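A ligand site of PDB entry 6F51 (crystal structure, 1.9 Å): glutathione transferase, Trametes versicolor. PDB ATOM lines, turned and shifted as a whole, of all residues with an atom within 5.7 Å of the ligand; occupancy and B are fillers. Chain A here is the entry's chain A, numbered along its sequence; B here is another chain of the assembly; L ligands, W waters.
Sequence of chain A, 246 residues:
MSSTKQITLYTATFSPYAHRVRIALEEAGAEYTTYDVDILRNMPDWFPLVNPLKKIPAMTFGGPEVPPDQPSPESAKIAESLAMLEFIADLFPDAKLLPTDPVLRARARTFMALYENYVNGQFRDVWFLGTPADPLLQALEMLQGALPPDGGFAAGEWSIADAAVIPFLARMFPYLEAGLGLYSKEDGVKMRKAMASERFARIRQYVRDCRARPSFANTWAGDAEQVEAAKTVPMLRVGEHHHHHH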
ATOM      1  N   PHE A  14      -5.669 -14.484  16.954  1.00  0.00           N
ATOM      2  CA  PHE A  14      -6.482 -15.087  18.004  1.00  0.00           C
ATOM      3  C   PHE A  14      -6.548 -16.625  17.944  1.00  0.00           C
ATOM      4  O   PHE A  14      -7.433 -17.208  18.577  1.00  0.00           O
ATOM      5  CB  PHE A  14      -7.900 -14.547  17.919  1.00  0.00           C
ATOM      6  CG  PHE A  14      -8.537 -14.812  16.586  1.00  0.00           C
ATOM      7  CD1 PHE A  14      -9.152 -16.040  16.338  1.00  0.00           C
ATOM      8  CD2 PHE A  14      -8.470 -13.852  15.560  1.00  0.00           C
ATOM      9  CE1 PHE A  14      -9.732 -16.297  15.111  1.00  0.00           C
ATOM     10  CE2 PHE A  14      -9.046 -14.116  14.309  1.00  0.00           C
ATOM     11  CZ  PHE A  14      -9.677 -15.343  14.080  1.00  0.00           C
ATOM     12  N   SER A  15      -5.713 -17.294  17.164  1.00  0.00           N
ATOM     13  CA  SER A  15      -5.747 -18.762  17.167  1.00  0.00           C
ATOM     14  C   SER A  15      -4.525 -19.308  17.908  1.00  0.00           C
ATOM     15  O   SER A  15      -3.414 -19.299  17.347  1.00  0.00           O
ATOM     16  CB  SER A  15      -5.780 -19.298  15.753  1.00  0.00           C
ATOM     17  OG  SER A  15      -5.645 -20.685  15.796  1.00  0.00           O
ATOM     18  N   PRO A  16      -4.678 -19.831  19.131  1.00  0.00           N
ATOM     19  CA  PRO A  16      -3.541 -20.505  19.766  1.00  0.00           C
ATOM     20  C   PRO A  16      -3.087 -21.706  18.996  1.00  0.00           C
ATOM     21  O   PRO A  16      -1.910 -22.086  19.094  1.00  0.00           O
ATOM     22  CB  PRO A  16      -4.082 -20.875  21.152  1.00  0.00           C
ATOM     23  CG  PRO A  16      -5.536 -20.893  21.005  1.00  0.00           C
ATOM     24  CD  PRO A  16      -5.912 -19.949  19.926  1.00  0.00           C
ATOM     25  N   TYR A  17      -3.954 -22.328  18.190  1.00  0.00           N
ATOM     26  CA  TYR A  17      -3.517 -23.452  17.361  1.00  0.00           C
ATOM     27  C   TYR A  17      -2.524 -23.011  16.306  1.00  0.00           C
ATOM     28  O   TYR A  17      -1.547 -23.705  16.034  1.00  0.00           O
ATOM     29  CB  TYR A  17      -4.723 -24.122  16.693  1.00  0.00           C
ATOM     30  CG  TYR A  17      -5.700 -24.673  17.679  1.00  0.00           C
ATOM     31  CD1 TYR A  17      -5.482 -25.893  18.273  1.00  0.00           C
ATOM     32  CD2 TYR A  17      -6.853 -23.942  18.053  1.00  0.00           C
ATOM     33  CE1 TYR A  17      -6.363 -26.404  19.195  1.00  0.00           C
ATOM     34  CE2 TYR A  17      -7.736 -24.430  18.973  1.00  0.00           C
ATOM     35  CZ  TYR A  17      -7.480 -25.672  19.540  1.00  0.00           C
ATOM     36  OH  TYR A  17      -8.324 -26.220  20.462  1.00  0.00           O
ATOM     37  N   ARG A  20       0.925 -22.293  17.756  1.00  0.00           N
ATOM     38  CA  ARG A  20       1.796 -23.460  17.936  1.00  0.00           C
ATOM     39  C   ARG A  20       2.752 -23.609  16.779  1.00  0.00           C
ATOM     40  O   ARG A  20       3.943 -23.907  16.946  1.00  0.00           O
ATOM     41  CB  ARG A  20       0.982 -24.757  17.997  1.00  0.00           C
ATOM     42  CG  ARG A  20       0.027 -24.914  19.089  1.00  0.00           C
ATOM     43  CD  ARG A  20      -0.859 -26.145  18.827  1.00  0.00           C
ATOM     44  NE  ARG A  20      -1.342 -26.643  20.104  1.00  0.00           N
ATOM     45  CZ  ARG A  20      -2.262 -27.601  20.309  1.00  0.00           C
ATOM     46  NH1 ARG A  20      -2.894 -28.193  19.305  1.00  0.00           N
ATOM     47  NH2 ARG A  20      -2.566 -27.925  21.562  1.00  0.00           N
ATOM     48  N   ILE A  39     -11.299 -16.135   9.874  1.00  0.00           N
ATOM     49  CA  ILE A  39     -12.034 -17.378   9.765  1.00  0.00           C
ATOM     50  C   ILE A  39     -13.368 -17.351  10.506  1.00  0.00           C
ATOM     51  O   ILE A  39     -14.298 -18.073  10.139  1.00  0.00           O
ATOM     52  CB  ILE A  39     -11.160 -18.537  10.278  1.00  0.00           C
ATOM     53  CG1 ILE A  39     -11.818 -19.868   9.910  1.00  0.00           C
ATOM     54  CG2 ILE A  39     -10.952 -18.470  11.794  1.00  0.00           C
ATOM     55  CD1 ILE A  39     -11.929 -20.131   8.367  1.00  0.00           C
ATOM     56  N   LEU A  40     -13.482 -16.592  11.574  1.00  0.00           N
ATOM     57  CA  LEU A  40     -14.678 -16.633  12.383  1.00  0.00           C
ATOM     58  C   LEU A  40     -15.741 -15.658  11.912  1.00  0.00           C
ATOM     59  O   LEU A  40     -16.925 -15.861  12.202  1.00  0.00           O
ATOM     60  CB  LEU A  40     -14.339 -16.335  13.855  1.00  0.00           C
ATOM     61  CG  LEU A  40     -13.256 -17.276  14.423  1.00  0.00           C
ATOM     62  CD1 LEU A  40     -12.922 -16.941  15.858  1.00  0.00           C
ATOM     63  CD2 LEU A  40     -13.689 -18.740  14.315  1.00  0.00           C
ATOM     64  N   LEU A  53     -11.985 -28.425   6.290  1.00  0.00           N
ATOM     65  CA  LEU A  53     -12.626 -28.286   7.588  1.00  0.00           C
ATOM     66  C   LEU A  53     -12.890 -26.849   7.969  1.00  0.00           C
ATOM     67  O   LEU A  53     -13.536 -26.610   8.984  1.00  0.00           O
ATOM     68  CB  LEU A  53     -11.758 -28.934   8.651  1.00  0.00           C
ATOM     69  CG  LEU A  53     -11.427 -30.383   8.396  1.00  0.00           C
ATOM     70  CD1 LEU A  53     -10.170 -30.727   9.167  1.00  0.00           C
ATOM     71  CD2 LEU A  53     -12.573 -31.254   8.830  1.00  0.00           C
ATOM     72  N   LYS A  54     -12.365 -25.899   7.194  1.00  0.00           N
ATOM     73  CA  LYS A  54     -12.612 -24.480   7.425  1.00  0.00           C
ATOM     74  C   LYS A  54     -12.106 -24.052   8.806  1.00  0.00           C
ATOM     75  O   LYS A  54     -12.795 -23.404   9.586  1.00  0.00           O
ATOM     76  CB  LYS A  54     -14.070 -24.113   7.241  1.00  0.00           C
ATOM     77  CG  LYS A  54     -14.598 -24.568   5.885  1.00  0.00           C
ATOM     78  CD  LYS A  54     -15.998 -24.074   5.598  1.00  0.00           C
ATOM     79  CE  LYS A  54     -17.068 -24.866   6.319  1.00  0.00           C
ATOM     80  NZ  LYS A  54     -18.430 -24.395   5.915  1.00  0.00           N
ATOM     81  N   LYS A  55     -10.863 -24.440   9.098  1.00  0.00           N
ATOM     82  CA  LYS A  55     -10.257 -24.067  10.361  1.00  0.00           C
ATOM     83  C   LYS A  55      -8.852 -23.550  10.160  1.00  0.00           C
ATOM     84  O   LYS A  55      -8.155 -23.930   9.211  1.00  0.00           O
ATOM     85  CB  LYS A  55     -10.238 -25.248  11.314  1.00  0.00           C
ATOM     86  CG  LYS A  55     -11.625 -25.620  11.841  1.00  0.00           C
ATOM     87  CD  LYS A  55     -11.514 -26.781  12.791  1.00  0.00           C
ATOM     88  CE  LYS A  55     -12.851 -27.224  13.373  1.00  0.00           C
ATOM     89  NZ  LYS A  55     -13.028 -28.574  12.854  1.00  0.00           N
ATOM     90  N   ILE A  56      -8.426 -22.698  11.098  1.00  0.00           N
ATOM     91  CA  ILE A  56      -7.093 -22.173  11.167  1.00  0.00           C
ATOM     92  C   ILE A  56      -6.374 -22.841  12.362  1.00  0.00           C
ATOM     93  O   ILE A  56      -6.943 -22.936  13.437  1.00  0.00           O
ATOM     94  CB  ILE A  56      -7.167 -20.635  11.329  1.00  0.00           C
ATOM     95  CG1 ILE A  56      -7.546 -20.010   9.988  1.00  0.00           C
ATOM     96  CG2 ILE A  56      -5.917 -20.032  11.998  1.00  0.00           C
ATOM     97  CD1 ILE A  56      -6.378 -19.945   9.042  1.00  0.00           C
ATOM     98  N   PRO A  57      -5.127 -23.262  12.174  1.00  0.00           N
ATOM     99  CA  PRO A  57      -4.358 -23.058  10.950  1.00  0.00           C
ATOM    100  C   PRO A  57      -4.657 -24.019   9.789  1.00  0.00           C
ATOM    101  O   PRO A  57      -5.208 -25.119   9.950  1.00  0.00           O
ATOM    102  CB  PRO A  57      -2.922 -23.308  11.407  1.00  0.00           C
ATOM    103  CG  PRO A  57      -3.095 -24.389  12.459  1.00  0.00           C
ATOM    104  CD  PRO A  57      -4.311 -23.936  13.210  1.00  0.00           C
ATOM    105  N   GLU A  80      -4.452 -29.732  10.766  1.00  0.00           N
ATOM    106  CA  GLU A  80      -4.327 -30.060  12.182  1.00  0.00           C
ATOM    107  C   GLU A  80      -2.961 -29.657  12.760  1.00  0.00           C
ATOM    108  O   GLU A  80      -1.942 -30.237  12.415  1.00  0.00           O
ATOM    109  CB  GLU A  80      -4.629 -31.547  12.408  1.00  0.00           C
ATOM    110  CG  GLU A  80      -6.107 -31.880  12.076  1.00  0.00           C
ATOM    111  CD  GLU A  80      -7.083 -31.156  12.971  1.00  0.00           C
ATOM    112  OE1 GLU A  80      -7.056 -31.346  14.211  1.00  0.00           O
ATOM    113  OE2 GLU A  80      -7.888 -30.395  12.432  1.00  0.00           O
ATOM    114  N   SER A  81      -2.990 -28.643  13.645  1.00  0.00           N
ATOM    115  CA  SER A  81      -1.780 -28.042  14.244  1.00  0.00           C
ATOM    116  C   SER A  81      -0.759 -29.069  14.744  1.00  0.00           C
ATOM    117  O   SER A  81       0.443 -28.899  14.539  1.00  0.00           O
ATOM    118  CB  SER A  81      -2.140 -27.098  15.390  1.00  0.00           C
ATOM    119  OG  SER A  81      -2.714 -27.758  16.513  1.00  0.00           O
ATOM    120  N   LEU A  82      -1.211 -30.147  15.391  1.00  0.00           N
ATOM    121  CA  LEU A  82      -0.224 -31.116  15.921  1.00  0.00           C
ATOM    122  C   LEU A  82       0.410 -31.953  14.816  1.00  0.00           C
ATOM    123  O   LEU A  82       1.578 -32.363  14.934  1.00  0.00           O
ATOM    124  CB  LEU A  82      -0.853 -32.040  16.955  1.00  0.00           C
ATOM    125  CG  LEU A  82      -1.305 -31.387  18.259  1.00  0.00           C
ATOM    126  CD1 LEU A  82      -1.731 -32.467  19.243  1.00  0.00           C
ATOM    127  CD2 LEU A  82      -0.260 -30.462  18.842  1.00  0.00           C
ATOM    128  N   MET A  84       1.027 -30.673  11.891  1.00  0.00           N
ATOM    129  CA  MET A  84       2.002 -29.707  11.401  1.00  0.00           C
ATOM    130  C   MET A  84       3.269 -29.694  12.245  1.00  0.00           C
ATOM    131  O   MET A  84       4.377 -29.689  11.697  1.00  0.00           O
ATOM    132  CB  MET A  84       1.374 -28.326  11.373  1.00  0.00           C
ATOM    133  CG  MET A  84       0.288 -28.187  10.327  1.00  0.00           C
ATOM    134  SD  MET A  84      -0.523 -26.602  10.434  1.00  0.00           S
ATOM    135  CE  MET A  84      -2.114 -26.952   9.688  1.00  0.00           C
ATOM    136  N   GLU A 116      -3.899 -32.035  25.137  1.00  0.00           N
ATOM    137  CA  GLU A 116      -5.019 -32.079  24.193  1.00  0.00           C
ATOM    138  C   GLU A 116      -6.222 -32.827  24.781  1.00  0.00           C
ATOM    139  O   GLU A 116      -7.361 -32.412  24.559  1.00  0.00           O
ATOM    140  CB  GLU A 116      -4.565 -32.728  22.876  1.00  0.00           C
ATOM    141  CG  GLU A 116      -5.181 -32.103  21.560  1.00  0.00           C
ATOM    142  CD  GLU A 116      -4.541 -30.771  21.151  1.00  0.00           C
ATOM    143  OE1 GLU A 116      -4.602 -30.396  19.943  1.00  0.00           O
ATOM    144  OE2 GLU A 116      -3.927 -30.113  21.995  1.00  0.00           O
ATOM    145  N   PHE A 123     -10.087 -25.535  29.317  1.00  0.00           N
ATOM    146  CA  PHE A 123      -9.938 -24.138  28.911  1.00  0.00           C
ATOM    147  C   PHE A 123     -11.126 -23.679  28.089  1.00  0.00           C
ATOM    148  O   PHE A 123     -11.705 -22.627  28.347  1.00  0.00           O
ATOM    149  CB  PHE A 123      -8.686 -23.960  28.098  1.00  0.00           C
ATOM    150  CG  PHE A 123      -7.486 -23.666  28.885  1.00  0.00           C
ATOM    151  CD1 PHE A 123      -7.476 -22.621  29.802  1.00  0.00           C
ATOM    152  CD2 PHE A 123      -6.332 -24.383  28.688  1.00  0.00           C
ATOM    153  CE1 PHE A 123      -6.335 -22.305  30.513  1.00  0.00           C
ATOM    154  CE2 PHE A 123      -5.181 -24.094  29.387  1.00  0.00           C
ATOM    155  CZ  PHE A 123      -5.172 -23.063  30.307  1.00  0.00           C
ATOM    156  N   ARG A 124     -11.486 -24.447  27.061  1.00  0.00           N
ATOM    157  CA  ARG A 124     -12.616 -24.044  26.208  1.00  0.00           C
ATOM    158  C   ARG A 124     -13.891 -23.876  27.022  1.00  0.00           C
ATOM    159  O   ARG A 124     -14.550 -22.834  26.973  1.00  0.00           O
ATOM    160  CB  ARG A 124     -12.860 -25.085  25.100  1.00  0.00           C
ATOM    161  CG  ARG A 124     -12.035 -24.871  23.870  1.00  0.00           C
ATOM    162  CD  ARG A 124     -12.000 -26.112  22.973  1.00  0.00           C
ATOM    163  NE  ARG A 124     -12.927 -26.070  21.844  1.00  0.00           N
ATOM    164  CZ  ARG A 124     -12.799 -26.816  20.745  1.00  0.00           C
ATOM    165  NH1 ARG A 124     -11.779 -27.668  20.645  1.00  0.00           N
ATOM    166  NH2 ARG A 124     -13.676 -26.727  19.752  1.00  0.00           N
ATOM    167  N   TRP A 127     -13.628 -20.836  29.542  1.00  0.00           N
ATOM    168  CA  TRP A 127     -13.566 -19.529  28.889  1.00  0.00           C
ATOM    169  C   TRP A 127     -14.785 -19.276  27.991  1.00  0.00           C
ATOM    170  O   TRP A 127     -15.285 -18.152  27.920  1.00  0.00           O
ATOM    171  CB  TRP A 127     -12.276 -19.401  28.088  1.00  0.00           C
ATOM    172  CG  TRP A 127     -11.321 -18.544  28.713  1.00  0.00           C
ATOM    173  CD1 TRP A 127     -10.959 -17.284  28.338  1.00  0.00           C
ATOM    174  CD2 TRP A 127     -10.542 -18.848  29.866  1.00  0.00           C
ATOM    175  NE1 TRP A 127     -10.024 -16.790  29.188  1.00  0.00           N
ATOM    176  CE2 TRP A 127      -9.747 -17.729  30.145  1.00  0.00           C
ATOM    177  CE3 TRP A 127     -10.445 -19.959  30.714  1.00  0.00           C
ATOM    178  CZ2 TRP A 127      -8.859 -17.685  31.235  1.00  0.00           C
ATOM    179  CZ3 TRP A 127      -9.583 -19.905  31.792  1.00  0.00           C
ATOM    180  CH2 TRP A 127      -8.800 -18.790  32.044  1.00  0.00           C
ATOM    181  N   PHE A 128     -15.262 -20.300  27.274  1.00  0.00           N
ATOM    182  CA  PHE A 128     -16.334 -20.070  26.308  1.00  0.00           C
ATOM    183  C   PHE A 128     -17.719 -20.319  26.882  1.00  0.00           C
ATOM    184  O   PHE A 128     -18.665 -19.675  26.452  1.00  0.00           O
ATOM    185  CB  PHE A 128     -16.193 -20.954  25.056  1.00  0.00           C
ATOM    186  CG  PHE A 128     -15.007 -20.626  24.228  1.00  0.00           C
ATOM    187  CD1 PHE A 128     -14.810 -19.365  23.731  1.00  0.00           C
ATOM    188  CD2 PHE A 128     -14.089 -21.595  23.939  1.00  0.00           C
ATOM    189  CE1 PHE A 128     -13.708 -19.071  22.972  1.00  0.00           C
ATOM    190  CE2 PHE A 128     -12.975 -21.295  23.184  1.00  0.00           C
ATOM    191  CZ  PHE A 128     -12.794 -20.033  22.705  1.00  0.00           C
ATOM    192  N   PRO A 167       0.962 -21.696  23.747  1.00  0.00           N
ATOM    193  CA  PRO A 167      -0.039 -20.711  23.301  1.00  0.00           C
ATOM    194  C   PRO A 167      -1.228 -20.632  24.210  1.00  0.00           C
ATOM    195  O   PRO A 167      -1.778 -19.549  24.439  1.00  0.00           O
ATOM    196  CB  PRO A 167      -0.425 -21.170  21.888  1.00  0.00           C
ATOM    197  CG  PRO A 167       0.788 -21.881  21.437  1.00  0.00           C
ATOM    198  CD  PRO A 167       1.244 -22.656  22.653  1.00  0.00           C
ATOM    199  N   PHE A 168      -1.625 -21.741  24.803  1.00  0.00           N
ATOM    200  CA  PHE A 168      -2.781 -21.673  25.665  1.00  0.00           C
ATOM    201  C   PHE A 168      -2.395 -21.177  27.072  1.00  0.00           C
ATOM    202  O   PHE A 168      -3.099 -20.340  27.650  1.00  0.00           O
ATOM    203  CB  PHE A 168      -3.469 -23.035  25.710  1.00  0.00           C
ATOM    204  CG  PHE A 168      -3.943 -23.494  24.351  1.00  0.00           C
ATOM    205  CD1 PHE A 168      -3.060 -24.074  23.455  1.00  0.00           C
ATOM    206  CD2 PHE A 168      -5.252 -23.295  23.965  1.00  0.00           C
ATOM    207  CE1 PHE A 168      -3.493 -24.489  22.216  1.00  0.00           C
ATOM    208  CE2 PHE A 168      -5.690 -23.691  22.736  1.00  0.00           C
ATOM    209  CZ  PHE A 168      -4.822 -24.281  21.849  1.00  0.00           C
ATOM    210  N   ARG A 171      -1.681 -17.381  27.054  1.00  0.00           N
ATOM    211  CA  ARG A 171      -2.898 -16.579  27.011  1.00  0.00           C
ATOM    212  C   ARG A 171      -3.658 -16.558  28.340  1.00  0.00           C
ATOM    213  O   ARG A 171      -4.374 -15.590  28.633  1.00  0.00           O
ATOM    214  CB  ARG A 171      -3.799 -17.095  25.924  1.00  0.00           C
ATOM    215  CG  ARG A 171      -3.370 -16.629  24.565  1.00  0.00           C
ATOM    216  CD  ARG A 171      -4.047 -17.509  23.529  1.00  0.00           C
ATOM    217  NE  ARG A 171      -3.827 -17.048  22.171  1.00  0.00           N
ATOM    218  CZ  ARG A 171      -2.705 -17.238  21.479  1.00  0.00           C
ATOM    219  NH1 ARG A 171      -1.687 -17.884  21.987  1.00  0.00           N
ATOM    220  NH2 ARG A 171      -2.629 -16.769  20.246  1.00  0.00           N
ATOM    221  N   MET A 172      -3.566 -17.631  29.128  1.00  0.00           N
ATOM    222  CA  MET A 172      -4.390 -17.713  30.325  1.00  0.00           C
ATOM    223  C   MET A 172      -4.182 -16.509  31.256  1.00  0.00           C
ATOM    224  O   MET A 172      -5.157 -15.963  31.797  1.00  0.00           O
ATOM    225  CB  MET A 172      -4.102 -18.993  31.084  1.00  0.00           C
ATOM    226  CG  MET A 172      -4.971 -19.193  32.277  1.00  0.00           C
ATOM    227  SD  MET A 172      -4.432 -20.572  33.313  1.00  0.00           S
ATOM    228  CE  MET A 172      -5.910 -20.725  34.287  1.00  0.00           C
ATOM    229  N   TYR A 175      -5.504 -13.016  29.803  1.00  0.00           N
ATOM    230  CA  TYR A 175      -6.971 -13.047  29.709  1.00  0.00           C
ATOM    231  C   TYR A 175      -7.617 -12.991  31.089  1.00  0.00           C
ATOM    232  O   TYR A 175      -8.700 -12.425  31.243  1.00  0.00           O
ATOM    233  CB  TYR A 175      -7.473 -14.307  29.007  1.00  0.00           C
ATOM    234  CG  TYR A 175      -7.145 -14.428  27.510  1.00  0.00           C
ATOM    235  CD1 TYR A 175      -6.264 -13.559  26.890  1.00  0.00           C
ATOM    236  CD2 TYR A 175      -7.704 -15.434  26.740  1.00  0.00           C
ATOM    237  CE1 TYR A 175      -5.962 -13.689  25.542  1.00  0.00           C
ATOM    238  CE2 TYR A 175      -7.395 -15.560  25.387  1.00  0.00           C
ATOM    239  CZ  TYR A 175      -6.531 -14.670  24.806  1.00  0.00           C
ATOM    240  OH  TYR A 175      -6.216 -14.771  23.469  1.00  0.00           O
ATOM    241  N   VAL A 233     -13.330 -12.593  18.854  1.00  0.00           N
ATOM    242  CA  VAL A 233     -13.877 -13.930  18.781  1.00  0.00           C
ATOM    243  C   VAL A 233     -15.326 -13.888  19.228  1.00  0.00           C
ATOM    244  O   VAL A 233     -15.583 -13.547  20.386  1.00  0.00           O
ATOM    245  CB  VAL A 233     -13.054 -14.894  19.647  1.00  0.00           C
ATOM    246  CG1 VAL A 233     -13.789 -16.221  19.854  1.00  0.00           C
ATOM    247  CG2 VAL A 233     -11.695 -15.103  19.001  1.00  0.00           C
ATOM    248  N   LEU A 236     -16.433 -15.726  22.333  1.00  0.00           N
ATOM    249  CA  LEU A 236     -16.092 -14.954  23.538  1.00  0.00           C
ATOM    250  C   LEU A 236     -16.965 -13.702  23.514  1.00  0.00           C
ATOM    251  O   LEU A 236     -16.539 -12.600  23.121  1.00  0.00           O
ATOM    252  CB  LEU A 236     -14.607 -14.595  23.593  1.00  0.00           C
ATOM    253  CG  LEU A 236     -13.650 -15.727  23.984  1.00  0.00           C
ATOM    254  CD1 LEU A 236     -12.225 -15.369  23.664  1.00  0.00           C
ATOM    255  CD2 LEU A 236     -13.778 -16.080  25.459  1.00  0.00           C
ATOM    256  N   ASN B 117      -9.814 -35.619  17.256  1.00  0.00           N
ATOM    257  CA  ASN B 117     -10.432 -34.326  17.529  1.00  0.00           C
ATOM    258  C   ASN B 117     -11.887 -34.232  17.118  1.00  0.00           C
ATOM    259  O   ASN B 117     -12.640 -33.526  17.785  1.00  0.00           O
ATOM    260  CB  ASN B 117      -9.642 -33.191  16.866  1.00  0.00           C
ATOM    261  CG  ASN B 117      -8.316 -32.965  17.569  1.00  0.00           C
ATOM    262  OD1 ASN B 117      -8.249 -33.107  18.793  1.00  0.00           O
ATOM    263  ND2 ASN B 117      -7.268 -32.658  16.822  1.00  0.00           N
ATOM    264  N   TYR B 118     -12.326 -34.951  16.076  1.00  0.00           N
ATOM    265  CA  TYR B 118     -13.688 -34.803  15.566  1.00  0.00           C
ATOM    266  C   TYR B 118     -14.539 -36.061  15.605  1.00  0.00           C
ATOM    267  O   TYR B 118     -15.768 -35.941  15.585  1.00  0.00           O
ATOM    268  CB  TYR B 118     -13.677 -34.255  14.127  1.00  0.00           C
ATOM    269  CG  TYR B 118     -12.727 -33.071  14.018  1.00  0.00           C
ATOM    270  CD1 TYR B 118     -12.911 -31.938  14.813  1.00  0.00           C
ATOM    271  CD2 TYR B 118     -11.611 -33.124  13.218  1.00  0.00           C
ATOM    272  CE1 TYR B 118     -12.016 -30.864  14.782  1.00  0.00           C
ATOM    273  CE2 TYR B 118     -10.726 -32.051  13.146  1.00  0.00           C
ATOM    274  CZ  TYR B 118     -10.920 -30.926  13.959  1.00  0.00           C
ATOM    275  OH  TYR B 118     -10.049 -29.847  13.962  1.00  0.00           O
HETATM  276  N1  LIG L   1      -7.700 -29.435  16.003  1.00  0.00           N
HETATM  277  C1  LIG L   1      -7.402 -28.188  15.234  1.00  0.00           C
HETATM  278  C2  LIG L   1      -5.885 -27.929  15.212  1.00  0.00           C
HETATM  279  O1  LIG L   1      -5.402 -27.273  14.268  1.00  0.00           O
HETATM  280  C3  LIG L   1      -8.220 -27.036  15.828  1.00  0.00           C
HETATM  281  C4  LIG L   1      -8.144 -25.761  15.028  1.00  0.00           C
HETATM  282  C5  LIG L   1      -9.236 -24.757  15.352  1.00  0.00           C
HETATM  283  O2  LIG L   1     -10.234 -25.071  15.996  1.00  0.00           O
HETATM  284  O3  LIG L   1      -5.232 -28.419  16.152  1.00  0.00           O
HETATM  285  N2  LIG L   1      -9.048 -23.537  14.865  1.00  0.00           N
HETATM  286  C6  LIG L   1      -9.924 -22.415  15.144  1.00  0.00           C
HETATM  287  C7  LIG L   1     -10.883 -22.200  13.969  1.00  0.00           C
HETATM  288  O4  LIG L   1     -10.430 -22.048  12.828  1.00  0.00           O
HETATM  289  C8  LIG L   1      -9.110 -21.158  15.426  1.00  0.00           C
HETATM  290  S1  LIG L   1     -10.206 -20.080  16.368  1.00  0.00           S
HETATM  291  C9  LIG L   1      -7.060 -19.851  24.774  1.00  0.00           C
HETATM  292  C10 LIG L   1      -6.658 -19.707  26.094  1.00  0.00           C
HETATM  293  C11 LIG L   1      -7.556 -19.902  27.109  1.00  0.00           C
HETATM  294  C12 LIG L   1      -8.849 -20.297  26.821  1.00  0.00           C
HETATM  295  C13 LIG L   1      -9.244 -20.471  25.502  1.00  0.00           C
HETATM  296  C14 LIG L   1      -8.366 -20.214  24.453  1.00  0.00           C
HETATM  297  C15 LIG L   1      -8.842 -20.158  23.047  1.00  0.00           C
HETATM  298  C16 LIG L   1      -9.129 -21.315  22.327  1.00  0.00           C
HETATM  299  C17 LIG L   1      -9.521 -21.243  20.990  1.00  0.00           C
HETATM  300  C18 LIG L   1      -9.647 -20.012  20.362  1.00  0.00           C
HETATM  301  C19 LIG L   1      -9.419 -18.868  21.102  1.00  0.00           C
HETATM  302  C20 LIG L   1      -8.991 -18.940  22.410  1.00  0.00           C
HETATM  303  O5  LIG L   1     -10.137 -18.615  18.525  1.00  0.00           O
HETATM  304  N3  LIG L   1     -12.182 -22.247  14.234  1.00  0.00           N
HETATM  305  C21 LIG L   1     -13.177 -22.195  13.181  1.00  0.00           C
HETATM  306  C22 LIG L   1     -14.172 -23.346  13.183  1.00  0.00           C
HETATM  307  C23 LIG L   1     -10.192 -20.925  17.999  1.00  0.00           C
HETATM  308  O6  LIG L   1     -13.938 -24.352  13.903  1.00  0.00           O
HETATM  309  C24 LIG L   1      -9.996 -19.754  18.941  1.00  0.00           C
HETATM  310  O7  LIG L   1     -15.188 -23.206  12.462  1.00  0.00           O
HETATM  311  O   HOH W   1      -4.050 -30.952  15.770  1.00  0.00           O
HETATM  312  O   HOH W   2      -6.280 -26.714  11.754  1.00  0.00           O
HETATM  313  O   HOH W   3     -15.259 -22.302  10.165  1.00  0.00           O
HETATM  314  O   HOH W   4      -7.128 -29.877  18.781  1.00  0.00           O
HETATM  315  O   HOH W   5     -11.929 -27.125  16.413  1.00  0.00           O
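Water W3 lies within hydrogen-bond range of an oxygen (O7) of the ligand (2.5 Å) and the backbone carbonyl oxygen (O) of Lys 54 (2.8 Å). Water W2 bridges the backbone carbonyl oxygen (O) of Pro 57 and an oxygen (O1) of the ligand. Water W1 lies within hydrogen-bond range of O3 of the ligand (2.8 Å), N of Leu 82 (3.0 Å), N of Ser 81 (3.3 Å) and OE1 of Glu 80 (3.4 Å). Water W4 lies within hydrogen-bond range of the side-chain carboxylate (OE1) of Glu 116, a nitrogen (N1) of the ligand and the side-chain amide nitrogen (ND2) of Asn 117 of chain B.
The backbone carbonyl oxygen (O) of Phe 14 lies close to an oxygen (O5) of the ligand (3.0 Å). OG of Ser 15 touches C8 of the ligand, at 3.5 Å. CD of Pro 16 touches C18 of the ligand (3.8 Å). CD1 of Tyr 17 touches O3 of the ligand, 3.3 Å away. Ile 39 touches the ligand (CG2 to O4, 3.8 Å). Leu 40 touches the ligand (CD2 to C21, 3.7 Å). Lys 54 touches the ligand. CE of Lys 55 touches O6 of the ligand, 3.1 Å away. CD of Pro 57 touches O1 of the ligand (3.7 Å). Phe 123 touches the ligand (CD1 to C11, 3.8 Å). Trp 127 touches the ligand. CZ of Phe 128 touches C17 of the ligand, 3.9 Å away. Phe 168 touches the ligand (O to C10, 3.9 Å). Arg 171 touches the ligand. CG2 of Val 233 touches O5 of the ligand (3.9 Å). Hydrophobic or aromatic side chains within 4 Å of the ligand: Phe 14, Pro 16, Tyr 17, Ile 39, Leu 40, Ile 56, Pro 57, Phe 123, Trp 127, Phe 128, Phe 168 and Val 233. The nearest printed residue that does not touch the ligand is Tyr 175 (4.3 Å).
The side-chain hydroxyl (OG) of Ser 81 is in hydrogen-bond range of the guanidinium group (NH1) of Arg 20 (2.8 Å). The side-chain carboxylate of Glu 80 lies within hydrogen-bond range of the side-chain hydroxyl of Tyr 118 of chain B (2.7 Å). ND2 of Asn 117 of chain B lies within hydrogen-bond range of OE1 of Glu 80 (2.9 Å). The side-chain hydroxyl of Tyr 118 of chain B sits close to the side-chain amino group of Lys 55 (3.4 Å). OG of Ser 15 lies close to N of Tyr 17, at 3.4 Å. NH1 of Arg 171 is in hydrogen-bond range of O of Pro 167, 3.0 Å away. OE2 of Glu 116 is in salt-bridge range of NH2 of Arg 20, at 2.6 Å.
The backbone NH of Ile 56 lies within hydrogen-bond range of an oxygen (O4) of the ligand (2.7 Å). The backbone carbonyl oxygen of Ile 56 lies within hydrogen-bond range of a nitrogen (N2) of the ligand (2.6 Å). N of Ser 81 is in hydrogen-bond range of O1 of the ligand, at 2.8 Å. An oxygen (O3) of the ligand sits at hydrogen-bond distance from the side-chain hydroxyl (OG) of Ser 81 (2.6 Å). OE1 of Glu 80 is in salt-bridge range of N1 of the ligand (2.7 Å). The side-chain hydroxyl (OH) of Tyr 118 of chain B sits at hydrogen-bond distance from a nitrogen (N1) of the ligand. The side-chain amide nitrogen (ND2) of Asn 117 of chain B lies close to a nitrogen (N1) of the ligand, at 3.4 Å. The guanidinium group (NH1) of Arg 20 lies within salt-bridge range of an oxygen (O3) of the ligand, at 3.9 Å.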
